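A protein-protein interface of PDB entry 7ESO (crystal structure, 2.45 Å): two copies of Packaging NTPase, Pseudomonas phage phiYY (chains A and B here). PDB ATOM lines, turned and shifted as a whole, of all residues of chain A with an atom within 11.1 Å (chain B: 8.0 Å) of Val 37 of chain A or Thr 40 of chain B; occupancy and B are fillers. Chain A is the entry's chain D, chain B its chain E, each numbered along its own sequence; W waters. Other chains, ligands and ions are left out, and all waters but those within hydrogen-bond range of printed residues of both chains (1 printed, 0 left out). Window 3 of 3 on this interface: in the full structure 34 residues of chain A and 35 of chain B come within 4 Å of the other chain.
NE of Arg 115 of chain B is in hydrogen-bond range of O of Pro 108 of chain A.
N of Val 37 of chain A is in hydrogen-bond range of OE2 of Glu 42 of chain B (3.2 Å).
The backbone NH (N) of Leu 35 of chain A is in hydrogen-bond range of the side-chain carboxylate (OE2) of Glu 42 of chain B, at 2.7 Å.
The backbone carbonyl oxygen of Leu 35 of chain A lies within hydrogen-bond range of the guanidinium group of Arg 115 of chain B, at 2.8 Å.
The backbone NH (N) of Val 36 of chain A is in hydrogen-bond range of the side-chain carboxylate (OE2) of Glu 42 of chain B, 2.8 Å away.
O of Ala 45 of chain B is in hydrogen-bond range of N of Leu 54 of chain B, at 2.9 Å.
N of Thr 40 of chain B lies within hydrogen-bond range of OE1 of Glu 44 of chain B (2.8 Å).
The side-chain carboxylate of Glu 38 of chain A is in salt-bridge range of the side-chain amino group of Lys 111 of chain A, at 3.7 Å.
NZ of Lys 111 of chain A lies within hydrogen-bond range of O of Val 109 of chain A (3.1 Å).
The backbone NH (N) of Glu 44 of chain B is in hydrogen-bond range of the side-chain hydroxyl (OG1) of Thr 41 of chain B, at 3.3 Å.
The backbone NH (N) of Ala 34 of chain A lies within hydrogen-bond range of the backbone carbonyl oxygen (O) of Arg 50 of chain A (2.9 Å).
Val 33 of chain A touches Glu 42 of chain B (O to OE1, 3.9 Å).
C of Ala 34 of chain A touches OE2 of Glu 42 of chain B, at 3.4 Å.
Leu 35 of chain A touches Ala 45 of chain B.
Leu 35 of chain A touches Leu 54 of chain B (O to CD1, 3.8 Å).
O of Ala 39 of chain B touches CG2 of Val 36 of chain A, at 3.7 Å.
CG1 of Val 36 of chain A touches O of Thr 41 of chain B, 3.6 Å away.
Thr 40 of chain B touches Val 37 of chain A.
Ala 107 of chain A touches Arg 115 of chain B.
Val 109 of chain A touches Arg 115 of chain B.
Lys 111 of chain A touches Arg 115 of chain B (NZ to NH1, 3.9 Å).
Of the printed residues of chain B, Val 36 of chain A touches Ala 39 (3.7 Å), Thr 41 (3.6 Å) and Glu 42 (2.8 Å).
Of the printed residues of chain B, Lys 111 of chain A touches Arg 115.
Ala 39 of chain B touches just one residue of chain A: Val 36.
Thr 40 of chain B touches one residue of chain A.
Thr 41 of chain B touches just one residue of chain A: Val 36 (3.6 Å).
No residue of chain A comes within 4 Å of Glu 44 of chain B.
Of the printed residues of chain A, Ala 45 of chain B touches Leu 35 (3.99 Å).
Of the printed residues of chain A, Leu 54 of chain B touches Leu 35.
The nearest printed residue of chain B that does not touch Ala 107 of chain A is Glu 42 of chain B (9.3 Å).
Printed residues of chain B that touch a printed residue of chain A: Ala 39, Thr 40, Thr 41, Glu 42, Ala 45, Leu 54 and Arg 115.
Hydrophobic or aromatic side chains of chain B that line the printed part of chain A: Ala 45 and Leu 54.
Of the 27 printed residues of chain A, 9 touch a printed residue of chain B.
Hydrophobic or aromatic side chains of chain A that line the printed part of chain B: Ala 34, Leu 35, Val 36, Val 37, Ala 107 and Val 109.
Among the printed residues, no Asp or Glu carboxylate lies within 4 Å of a Lys or Arg side-chain nitrogen of the other chain.
Val 37 of chain A touches Thr 40 of chain B, but with the chains exchanged Thr 40 of chain A does not touch Val 37 of chain B (18.8 Å).
Water W1 lies within hydrogen-bond range of O of Ala 107 of chain A, O of Ala 34 of chain A and NH2 of Arg 115 of chain B.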
ATOM      1  N   THR A  32      20.448 -10.777  21.668  1.00  0.00           N
ATOM      2  CA  THR A  32      21.477 -10.244  20.780  1.00  0.00           C
ATOM      3  C   THR A  32      20.846  -9.530  19.578  1.00  0.00           C
ATOM      4  O   THR A  32      21.508  -9.304  18.559  1.00  0.00           O
ATOM      5  CB  THR A  32      22.446 -11.367  20.289  1.00  0.00           C
ATOM      6  OG1 THR A  32      23.591 -10.785  19.656  1.00  0.00           O
ATOM      7  CG2 THR A  32      21.761 -12.318  19.313  1.00  0.00           C
ATOM      8  N   VAL A  33      19.565  -9.175  19.703  1.00  0.00           N
ATOM      9  CA  VAL A  33      18.870  -8.360  18.705  1.00  0.00           C
ATOM     10  C   VAL A  33      19.163  -6.884  18.952  1.00  0.00           C
ATOM     11  O   VAL A  33      19.022  -6.390  20.081  1.00  0.00           O
ATOM     12  CB  VAL A  33      17.356  -8.631  18.725  1.00  0.00           C
ATOM     13  CG1 VAL A  33      16.614  -7.609  17.889  1.00  0.00           C
ATOM     14  CG2 VAL A  33      17.082  -9.995  18.135  1.00  0.00           C
ATOM     15  N   ALA A  34      19.558  -6.175  17.887  1.00  0.00           N
ATOM     16  CA  ALA A  34      19.806  -4.738  17.973  1.00  0.00           C
ATOM     17  C   ALA A  34      18.529  -3.994  18.333  1.00  0.00           C
ATOM     18  O   ALA A  34      17.516  -4.107  17.637  1.00  0.00           O
ATOM     19  CB  ALA A  34      20.352  -4.211  16.649  1.00  0.00           C
ATOM     20  N   LEU A  35      18.583  -3.218  19.416  1.00  0.00           N
ATOM     21  CA  LEU A  35      17.412  -2.511  19.907  1.00  0.00           C
ATOM     22  C   LEU A  35      17.393  -1.023  19.588  1.00  0.00           C
ATOM     23  O   LEU A  35      16.306  -0.437  19.577  1.00  0.00           O
ATOM     24  CB  LEU A  35      17.283  -2.687  21.424  1.00  0.00           C
ATOM     25  CG  LEU A  35      17.006  -4.120  21.871  1.00  0.00           C
ATOM     26  CD1 LEU A  35      16.856  -4.145  23.368  1.00  0.00           C
ATOM     27  CD2 LEU A  35      15.770  -4.702  21.189  1.00  0.00           C
ATOM     28  N   VAL A  36      18.541  -0.398  19.313  1.00  0.00           N
ATOM     29  CA  VAL A  36      18.557   1.055  19.138  1.00  0.00           C
ATOM     30  C   VAL A  36      19.519   1.497  18.036  1.00  0.00           C
ATOM     31  O   VAL A  36      19.249   2.471  17.324  1.00  0.00           O
ATOM     32  CB  VAL A  36      18.879   1.750  20.478  1.00  0.00           C
ATOM     33  CG1 VAL A  36      20.337   1.513  20.881  1.00  0.00           C
ATOM     34  CG2 VAL A  36      18.578   3.238  20.402  1.00  0.00           C
ATOM     35  N   VAL A  37      20.634   0.795  17.867  1.00  0.00           N
ATOM     36  CA  VAL A  37      21.658   1.194  16.907  1.00  0.00           C
ATOM     37  C   VAL A  37      21.330   0.574  15.552  1.00  0.00           C
ATOM     38  O   VAL A  37      21.243  -0.650  15.420  1.00  0.00           O
ATOM     39  CB  VAL A  37      23.058   0.778  17.381  1.00  0.00           C
ATOM     40  CG1 VAL A  37      24.068   1.036  16.294  1.00  0.00           C
ATOM     41  CG2 VAL A  37      23.440   1.536  18.652  1.00  0.00           C
ATOM     42  N   GLU A  38      21.149   1.408  14.540  1.00  0.00           N
ATOM     43  CA  GLU A  38      20.788   0.903  13.227  1.00  0.00           C
ATOM     44  C   GLU A  38      21.837   1.300  12.200  1.00  0.00           C
ATOM     45  O   GLU A  38      22.617   2.234  12.403  1.00  0.00           O
ATOM     46  CB  GLU A  38      19.408   1.407  12.800  1.00  0.00           C
ATOM     47  CG  GLU A  38      19.365   2.866  12.409  1.00  0.00           C
ATOM     48  CD  GLU A  38      17.948   3.347  12.110  1.00  0.00           C
ATOM     49  OE1 GLU A  38      17.379   4.068  12.967  1.00  0.00           O
ATOM     50  OE2 GLU A  38      17.414   3.006  11.024  1.00  0.00           O
ATOM     51  N   ALA A  39      21.846   0.563  11.091  1.00  0.00           N
ATOM     52  CA  ALA A  39      22.828   0.777  10.036  1.00  0.00           C
ATOM     53  C   ALA A  39      22.843   2.227   9.563  1.00  0.00           C
ATOM     54  O   ALA A  39      21.793   2.819   9.298  1.00  0.00           O
ATOM     55  CB  ALA A  39      22.531  -0.147   8.859  1.00  0.00           C
ATOM     56  N   THR A  40      24.046   2.795   9.454  1.00  0.00           N
ATOM     57  CA  THR A  40      24.241   4.106   8.849  1.00  0.00           C
ATOM     58  C   THR A  40      25.207   4.091   7.671  1.00  0.00           C
ATOM     59  O   THR A  40      25.387   5.130   7.030  1.00  0.00           O
ATOM     60  CB  THR A  40      24.734   5.120   9.895  1.00  0.00           C
ATOM     61  OG1 THR A  40      26.064   4.778  10.318  1.00  0.00           O
ATOM     62  CG2 THR A  40      23.801   5.133  11.110  1.00  0.00           C
ATOM     63  N   THR A  41      25.833   2.960   7.368  1.00  0.00           N
ATOM     64  CA  THR A  41      26.662   2.831   6.181  1.00  0.00           C
ATOM     65  C   THR A  41      26.128   1.708   5.307  1.00  0.00           C
ATOM     66  O   THR A  41      25.366   0.842   5.753  1.00  0.00           O
ATOM     67  CB  THR A  41      28.138   2.551   6.529  1.00  0.00           C
ATOM     68  OG1 THR A  41      28.282   1.198   6.997  1.00  0.00           O
ATOM     69  CG2 THR A  41      28.651   3.537   7.592  1.00  0.00           C
ATOM     70  N   GLU A  44      27.061  -1.666   6.790  1.00  0.00           N
ATOM     71  CA  GLU A  44      26.194  -2.114   7.871  1.00  0.00           C
ATOM     72  C   GLU A  44      24.780  -2.396   7.383  1.00  0.00           C
ATOM     73  O   GLU A  44      24.110  -3.287   7.922  1.00  0.00           O
ATOM     74  CB  GLU A  44      26.168  -1.066   8.977  1.00  0.00           C
ATOM     75  CG  GLU A  44      27.477  -0.927   9.709  1.00  0.00           C
ATOM     76  CD  GLU A  44      27.582   0.379  10.480  1.00  0.00           C
ATOM     77  OE1 GLU A  44      26.772   1.298  10.216  1.00  0.00           O
ATOM     78  OE2 GLU A  44      28.473   0.481  11.355  1.00  0.00           O
ATOM     79  N   ALA A  45      24.308  -1.653   6.378  1.00  0.00           N
ATOM     80  CA  ALA A  45      22.960  -1.884   5.865  1.00  0.00           C
ATOM     81  C   ALA A  45      22.783  -3.288   5.305  1.00  0.00           C
ATOM     82  O   ALA A  45      21.660  -3.796   5.288  1.00  0.00           O
ATOM     83  CB  ALA A  45      22.606  -0.859   4.788  1.00  0.00           C
ATOM     84  N   LYS A  47      23.937  -6.072   6.644  1.00  0.00           N
ATOM     85  CA  LYS A  47      23.832  -7.093   7.667  1.00  0.00           C
ATOM     86  C   LYS A  47      22.365  -7.489   7.854  1.00  0.00           C
ATOM     87  O   LYS A  47      21.442  -6.860   7.318  1.00  0.00           O
ATOM     88  CB  LYS A  47      24.453  -6.599   8.978  1.00  0.00           C
ATOM     89  CG  LYS A  47      25.977  -6.356   8.916  1.00  0.00           C
ATOM     90  CD  LYS A  47      26.539  -5.885  10.271  1.00  0.00           C
ATOM     91  CE  LYS A  47      25.763  -4.664  10.804  1.00  0.00           C
ATOM     92  NZ  LYS A  47      26.289  -4.100  12.093  1.00  0.00           N
ATOM     93  N   SER A  48      22.160  -8.558   8.619  1.00  0.00           N
ATOM     94  CA  SER A  48      20.832  -9.083   8.872  1.00  0.00           C
ATOM     95  C   SER A  48      19.981  -8.074   9.649  1.00  0.00           C
ATOM     96  O   SER A  48      20.478  -7.081  10.196  1.00  0.00           O
ATOM     97  CB  SER A  48      20.929 -10.386   9.656  1.00  0.00           C
ATOM     98  OG  SER A  48      21.395 -10.112  10.969  1.00  0.00           O
ATOM     99  N   LEU A  49      18.677  -8.356   9.714  1.00  0.00           N
ATOM    100  CA  LEU A  49      17.777  -7.499  10.481  1.00  0.00           C
ATOM    101  C   LEU A  49      18.123  -7.539  11.962  1.00  0.00           C
ATOM    102  O   LEU A  49      18.054  -6.513  12.654  1.00  0.00           O
ATOM    103  CB  LEU A  49      16.327  -7.926  10.263  1.00  0.00           C
ATOM    104  CG  LEU A  49      15.870  -7.892   8.807  1.00  0.00           C
ATOM    105  CD1 LEU A  49      14.465  -8.400   8.707  1.00  0.00           C
ATOM    106  CD2 LEU A  49      15.966  -6.485   8.243  1.00  0.00           C
ATOM    107  N   ARG A  50      18.508  -8.721  12.459  1.00  0.00           N
ATOM    108  CA  ARG A  50      18.895  -8.872  13.859  1.00  0.00           C
ATOM    109  C   ARG A  50      20.024  -7.919  14.222  1.00  0.00           C
ATOM    110  O   ARG A  50      20.001  -7.289  15.287  1.00  0.00           O
ATOM    111  CB  ARG A  50      19.304 -10.324  14.134  1.00  0.00           C
ATOM    112  CG  ARG A  50      20.250 -10.511  15.314  1.00  0.00           C
ATOM    113  CD  ARG A  50      20.671 -11.974  15.497  1.00  0.00           C
ATOM    114  NE  ARG A  50      19.529 -12.881  15.446  1.00  0.00           N
ATOM    115  CZ  ARG A  50      18.748 -13.176  16.482  1.00  0.00           C
ATOM    116  NH1 ARG A  50      18.976 -12.637  17.671  1.00  0.00           N
ATOM    117  NH2 ARG A  50      17.728 -14.013  16.326  1.00  0.00           N
ATOM    118  N   GLU A  51      21.003  -7.779  13.337  1.00  0.00           N
ATOM    119  CA  GLU A  51      22.132  -6.892  13.554  1.00  0.00           C
ATOM    120  C   GLU A  51      21.837  -5.435  13.210  1.00  0.00           C
ATOM    121  O   GLU A  51      22.757  -4.614  13.260  1.00  0.00           O
ATOM    122  CB  GLU A  51      23.330  -7.364  12.733  1.00  0.00           C
ATOM    123  CG  GLU A  51      23.661  -8.836  12.867  1.00  0.00           C
ATOM    124  CD  GLU A  51      24.745  -9.272  11.883  1.00  0.00           C
ATOM    125  OE1 GLU A  51      24.396  -9.704  10.756  1.00  0.00           O
ATOM    126  OE2 GLU A  51      25.945  -9.166  12.232  1.00  0.00           O
ATOM    127  N   GLY A  52      20.608  -5.084  12.848  1.00  0.00           N
ATOM    128  CA  GLY A  52      20.301  -3.708  12.512  1.00  0.00           C
ATOM    129  C   GLY A  52      20.490  -3.339  11.059  1.00  0.00           C
ATOM    130  O   GLY A  52      20.431  -2.148  10.726  1.00  0.00           O
ATOM    131  N   GLY A  53      20.723  -4.314  10.185  1.00  0.00           N
ATOM    132  CA  GLY A  53      20.761  -4.066   8.762  1.00  0.00           C
ATOM    133  C   GLY A  53      19.365  -3.999   8.162  1.00  0.00           C
ATOM    134  O   GLY A  53      18.348  -3.975   8.855  1.00  0.00           O
ATOM    135  N   LEU A  54      19.334  -3.970   6.829  1.00  0.00           N
ATOM    136  CA  LEU A  54      18.106  -3.826   6.055  1.00  0.00           C
ATOM    137  C   LEU A  54      17.878  -4.985   5.092  1.00  0.00           C
ATOM    138  O   LEU A  54      16.890  -4.968   4.349  1.00  0.00           O
ATOM    139  CB  LEU A  54      18.123  -2.505   5.265  1.00  0.00           C
ATOM    140  CG  LEU A  54      18.020  -1.167   6.023  1.00  0.00           C
ATOM    141  CD1 LEU A  54      18.771  -0.055   5.301  1.00  0.00           C
ATOM    142  CD2 LEU A  54      16.574  -0.752   6.183  1.00  0.00           C
ATOM    143  N   PHE A 106      10.882 -10.785  16.623  1.00  0.00           N
ATOM    144  CA  PHE A 106      11.313  -9.491  17.120  1.00  0.00           C
ATOM    145  C   PHE A 106      10.947  -8.440  16.081  1.00  0.00           C
ATOM    146  O   PHE A 106      10.537  -8.761  14.963  1.00  0.00           O
ATOM    147  CB  PHE A 106      12.821  -9.485  17.401  1.00  0.00           C
ATOM    148  CG  PHE A 106      13.662  -9.710  16.176  1.00  0.00           C
ATOM    149  CD1 PHE A 106      13.905 -10.996  15.709  1.00  0.00           C
ATOM    150  CD2 PHE A 106      14.203  -8.639  15.484  1.00  0.00           C
ATOM    151  CE1 PHE A 106      14.678 -11.202  14.589  1.00  0.00           C
ATOM    152  CE2 PHE A 106      14.980  -8.842  14.353  1.00  0.00           C
ATOM    153  CZ  PHE A 106      15.219 -10.119  13.909  1.00  0.00           C
ATOM    154  N   ALA A 107      11.119  -7.175  16.452  1.00  0.00           N
ATOM    155  CA  ALA A 107      10.858  -6.060  15.545  1.00  0.00           C
ATOM    156  C   ALA A 107      12.174  -5.420  15.132  1.00  0.00           C
ATOM    157  O   ALA A 107      12.844  -4.803  15.977  1.00  0.00           O
ATOM    158  CB  ALA A 107       9.952  -5.026  16.212  1.00  0.00           C
ATOM    159  N   PRO A 108      12.583  -5.530  13.865  1.00  0.00           N
ATOM    160  CA  PRO A 108      13.858  -4.935  13.439  1.00  0.00           C
ATOM    161  C   PRO A 108      13.929  -3.454  13.767  1.00  0.00           C
ATOM    162  O   PRO A 108      12.912  -2.766  13.851  1.00  0.00           O
ATOM    163  CB  PRO A 108      13.871  -5.164  11.925  1.00  0.00           C
ATOM    164  CG  PRO A 108      12.978  -6.355  11.711  1.00  0.00           C
ATOM    165  CD  PRO A 108      11.949  -6.335  12.808  1.00  0.00           C
ATOM    166  N   VAL A 109      15.157  -2.967  13.946  1.00  0.00           N
ATOM    167  CA  VAL A 109      15.368  -1.574  14.332  1.00  0.00           C
ATOM    168  C   VAL A 109      15.516  -0.637  13.126  1.00  0.00           C
ATOM    169  O   VAL A 109      15.200   0.553  13.232  1.00  0.00           O
ATOM    170  CB  VAL A 109      16.585  -1.464  15.273  1.00  0.00           C
ATOM    171  CG1 VAL A 109      17.874  -1.797  14.531  1.00  0.00           C
ATOM    172  CG2 VAL A 109      16.667  -0.073  15.886  1.00  0.00           C
ATOM    173  N   ALA A 110      15.961  -1.140  11.973  1.00  0.00           N
ATOM    174  CA  ALA A 110      16.253  -0.266  10.837  1.00  0.00           C
ATOM    175  C   ALA A 110      14.982   0.400  10.308  1.00  0.00           C
ATOM    176  O   ALA A 110      14.018  -0.281   9.945  1.00  0.00           O
ATOM    177  CB  ALA A 110      16.939  -1.061   9.722  1.00  0.00           C
ATOM    178  N   LYS A 111      14.993   1.737  10.235  1.00  0.00           N
ATOM    179  CA  LYS A 111      13.790   2.487   9.877  1.00  0.00           C
ATOM    180  C   LYS A 111      13.439   2.399   8.396  1.00  0.00           C
ATOM    181  O   LYS A 111      12.276   2.604   8.042  1.00  0.00           O
ATOM    182  CB  LYS A 111      13.930   3.965  10.269  1.00  0.00           C
ATOM    183  CG  LYS A 111      14.051   4.212  11.774  1.00  0.00           C
ATOM    184  CD  LYS A 111      13.099   3.295  12.559  1.00  0.00           C
ATOM    185  CE  LYS A 111      13.068   3.614  14.060  1.00  0.00           C
ATOM    186  NZ  LYS A 111      14.265   3.058  14.796  1.00  0.00           N
ATOM    187  N   GLY A 112      14.391   2.095   7.526  1.00  0.00           N
ATOM    188  CA  GLY A 112      14.069   2.152   6.113  1.00  0.00           C
ATOM    189  C   GLY A 112      13.396   0.936   5.510  1.00  0.00           C
ATOM    190  O   GLY A 112      13.238   0.872   4.285  1.00  0.00           O
ATOM    191  N   VAL B  37      17.283  11.659  29.230  1.00  0.00           N
ATOM    192  CA  VAL B  37      18.399  10.935  28.635  1.00  0.00           C
ATOM    193  C   VAL B  37      17.984   9.481  28.454  1.00  0.00           C
ATOM    194  O   VAL B  37      17.658   8.793  29.428  1.00  0.00           O
ATOM    195  CB  VAL B  37      19.661  11.060  29.497  1.00  0.00           C
ATOM    196  CG1 VAL B  37      20.789  10.209  28.921  1.00  0.00           C
ATOM    197  CG2 VAL B  37      20.067  12.523  29.596  1.00  0.00           C
ATOM    198  N   GLU B  38      17.971   9.020  27.210  1.00  0.00           N
ATOM    199  CA  GLU B  38      17.553   7.667  26.886  1.00  0.00           C
ATOM    200  C   GLU B  38      18.708   6.913  26.246  1.00  0.00           C
ATOM    201  O   GLU B  38      19.686   7.506  25.784  1.00  0.00           O
ATOM    202  CB  GLU B  38      16.348   7.659  25.941  1.00  0.00           C
ATOM    203  CG  GLU B  38      16.676   8.173  24.555  1.00  0.00           C
ATOM    204  CD  GLU B  38      15.459   8.237  23.633  1.00  0.00           C
ATOM    205  OE1 GLU B  38      14.738   7.218  23.509  1.00  0.00           O
ATOM    206  OE2 GLU B  38      15.216   9.326  23.051  1.00  0.00           O
ATOM    207  N   ALA B  39      18.571   5.590  26.227  1.00  0.00           N
ATOM    208  CA  ALA B  39      19.602   4.723  25.678  1.00  0.00           C
ATOM    209  C   ALA B  39      20.008   5.157  24.278  1.00  0.00           C
ATOM    210  O   ALA B  39      19.168   5.386  23.406  1.00  0.00           O
ATOM    211  CB  ALA B  39      19.108   3.275  25.651  1.00  0.00           C
ATOM    212  N   THR B  40      21.310   5.272  24.074  1.00  0.00           N
ATOM    213  CA  THR B  40      21.855   5.551  22.762  1.00  0.00           C
ATOM    214  C   THR B  40      22.783   4.449  22.262  1.00  0.00           C
ATOM    215  O   THR B  40      23.116   4.437  21.075  1.00  0.00           O
ATOM    216  CB  THR B  40      22.589   6.902  22.772  1.00  0.00           C
ATOM    217  OG1 THR B  40      23.030   7.219  21.451  1.00  0.00           O
ATOM    218  CG2 THR B  40      23.786   6.867  23.702  1.00  0.00           C
ATOM    219  N   THR B  41      23.188   3.515  23.121  1.00  0.00           N
ATOM    220  CA  THR B  41      23.987   2.368  22.721  1.00  0.00           C
ATOM    221  C   THR B  41      23.265   1.079  23.093  1.00  0.00           C
ATOM    222  O   THR B  41      22.323   1.065  23.898  1.00  0.00           O
ATOM    223  CB  THR B  41      25.385   2.373  23.370  1.00  0.00           C
ATOM    224  OG1 THR B  41      25.272   2.176  24.788  1.00  0.00           O
ATOM    225  CG2 THR B  41      26.103   3.680  23.089  1.00  0.00           C
ATOM    226  N   GLU B  42      23.722  -0.014  22.478  1.00  0.00           N
ATOM    227  CA  GLU B  42      23.099  -1.307  22.722  1.00  0.00           C
ATOM    228  C   GLU B  42      23.244  -1.725  24.174  1.00  0.00           C
ATOM    229  O   GLU B  42      22.330  -2.349  24.732  1.00  0.00           O
ATOM    230  CB  GLU B  42      23.705  -2.357  21.793  1.00  0.00           C
ATOM    231  CG  GLU B  42      23.105  -2.314  20.392  1.00  0.00           C
ATOM    232  CD  GLU B  42      21.587  -2.497  20.386  1.00  0.00           C
ATOM    233  OE1 GLU B  42      21.050  -3.215  21.267  1.00  0.00           O
ATOM    234  OE2 GLU B  42      20.934  -1.905  19.498  1.00  0.00           O
ATOM    235  N   ALA B  43      24.366  -1.374  24.810  1.00  0.00           N
ATOM    236  CA  ALA B  43      24.544  -1.701  26.221  1.00  0.00           C
ATOM    237  C   ALA B  43      23.575  -0.912  27.095  1.00  0.00           C
ATOM    238  O   ALA B  43      23.010  -1.456  28.052  1.00  0.00           O
ATOM    239  CB  ALA B  43      25.993  -1.447  26.639  1.00  0.00           C
ATOM    240  N   GLU B  44      23.358   0.366  26.774  1.00  0.00           N
ATOM    241  CA  GLU B  44      22.370   1.148  27.513  1.00  0.00           C
ATOM    242  C   GLU B  44      20.951   0.642  27.269  1.00  0.00           C
ATOM    243  O   GLU B  44      20.124   0.658  28.188  1.00  0.00           O
ATOM    244  CB  GLU B  44      22.478   2.625  27.137  1.00  0.00           C
ATOM    245  CG  GLU B  44      23.765   3.283  27.602  1.00  0.00           C
ATOM    246  CD  GLU B  44      23.991   4.650  26.967  1.00  0.00           C
ATOM    247  OE1 GLU B  44      23.136   5.093  26.166  1.00  0.00           O
ATOM    248  OE2 GLU B  44      25.028   5.282  27.270  1.00  0.00           O
ATOM    249  N   ALA B  45      20.652   0.188  26.048  1.00  0.00           N
ATOM    250  CA  ALA B  45      19.313  -0.308  25.766  1.00  0.00           C
ATOM    251  C   ALA B  45      18.946  -1.511  26.633  1.00  0.00           C
ATOM    252  O   ALA B  45      17.756  -1.751  26.855  1.00  0.00           O
ATOM    253  CB  ALA B  45      19.179  -0.645  24.280  1.00  0.00           C
ATOM    254  N   LYS B  47      19.469  -1.724  29.798  1.00  0.00           N
ATOM    255  CA  LYS B  47      19.125  -1.286  31.137  1.00  0.00           C
ATOM    256  C   LYS B  47      17.601  -1.193  31.301  1.00  0.00           C
ATOM    257  O   LYS B  47      16.824  -1.257  30.339  1.00  0.00           O
ATOM    258  CB  LYS B  47      19.795   0.055  31.439  1.00  0.00           C
ATOM    259  CG  LYS B  47      21.323  -0.021  31.639  1.00  0.00           C
ATOM    260  CD  LYS B  47      21.878   1.303  32.181  1.00  0.00           C
ATOM    261  CE  LYS B  47      22.469   2.165  31.064  1.00  0.00           C
ATOM    262  NZ  LYS B  47      22.186   3.634  31.210  1.00  0.00           N
ATOM    263  N   GLY B  52      16.326   4.577  31.547  1.00  0.00           N
ATOM    264  CA  GLY B  52      16.352   5.055  30.183  1.00  0.00           C
ATOM    265  C   GLY B  52      16.518   3.979  29.137  1.00  0.00           C
ATOM    266  O   GLY B  52      16.609   4.308  27.943  1.00  0.00           O
ATOM    267  N   GLY B  53      16.561   2.705  29.543  1.00  0.00           N
ATOM    268  CA  GLY B  53      16.711   1.600  28.621  1.00  0.00           C
ATOM    269  C   GLY B  53      15.392   1.135  28.027  1.00  0.00           C
ATOM    270  O   GLY B  53      14.326   1.719  28.238  1.00  0.00           O
ATOM    271  N   LEU B  54      15.479   0.041  27.274  1.00  0.00           N
ATOM    272  CA  LEU B  54      14.347  -0.507  26.541  1.00  0.00           C
ATOM    273  C   LEU B  54      13.924  -1.884  27.043  1.00  0.00           C
ATOM    274  O   LEU B  54      13.049  -2.513  26.431  1.00  0.00           O
ATOM    275  CB  LEU B  54      14.683  -0.575  25.046  1.00  0.00           C
ATOM    276  CG  LEU B  54      14.808   0.769  24.330  1.00  0.00           C
ATOM    277  CD1 LEU B  54      15.779   0.668  23.184  1.00  0.00           C
ATOM    278  CD2 LEU B  54      13.447   1.190  23.812  1.00  0.00           C
ATOM    279  N   ARG B 115       7.847   0.249  19.055  1.00  0.00           N
ATOM    280  CA  ARG B 115       8.308  -0.684  18.039  1.00  0.00           C
ATOM    281  C   ARG B 115       8.684  -2.023  18.650  1.00  0.00           C
ATOM    282  O   ARG B 115       8.290  -3.076  18.135  1.00  0.00           O
ATOM    283  CB  ARG B 115       9.495  -0.089  17.283  1.00  0.00           C
ATOM    284  CG  ARG B 115       9.991  -0.972  16.166  1.00  0.00           C
ATOM    285  CD  ARG B 115      11.381  -0.588  15.769  1.00  0.00           C
ATOM    286  NE  ARG B 115      12.381  -1.259  16.590  1.00  0.00           N
ATOM    287  CZ  ARG B 115      13.167  -0.636  17.462  1.00  0.00           C
ATOM    288  NH1 ARG B 115      13.071   0.678  17.637  1.00  0.00           N
ATOM    289  NH2 ARG B 115      14.050  -1.331  18.156  1.00  0.00           N
HETATM  290  O   HOH W   1      14.800  -4.153  17.640  1.00  0.00           O
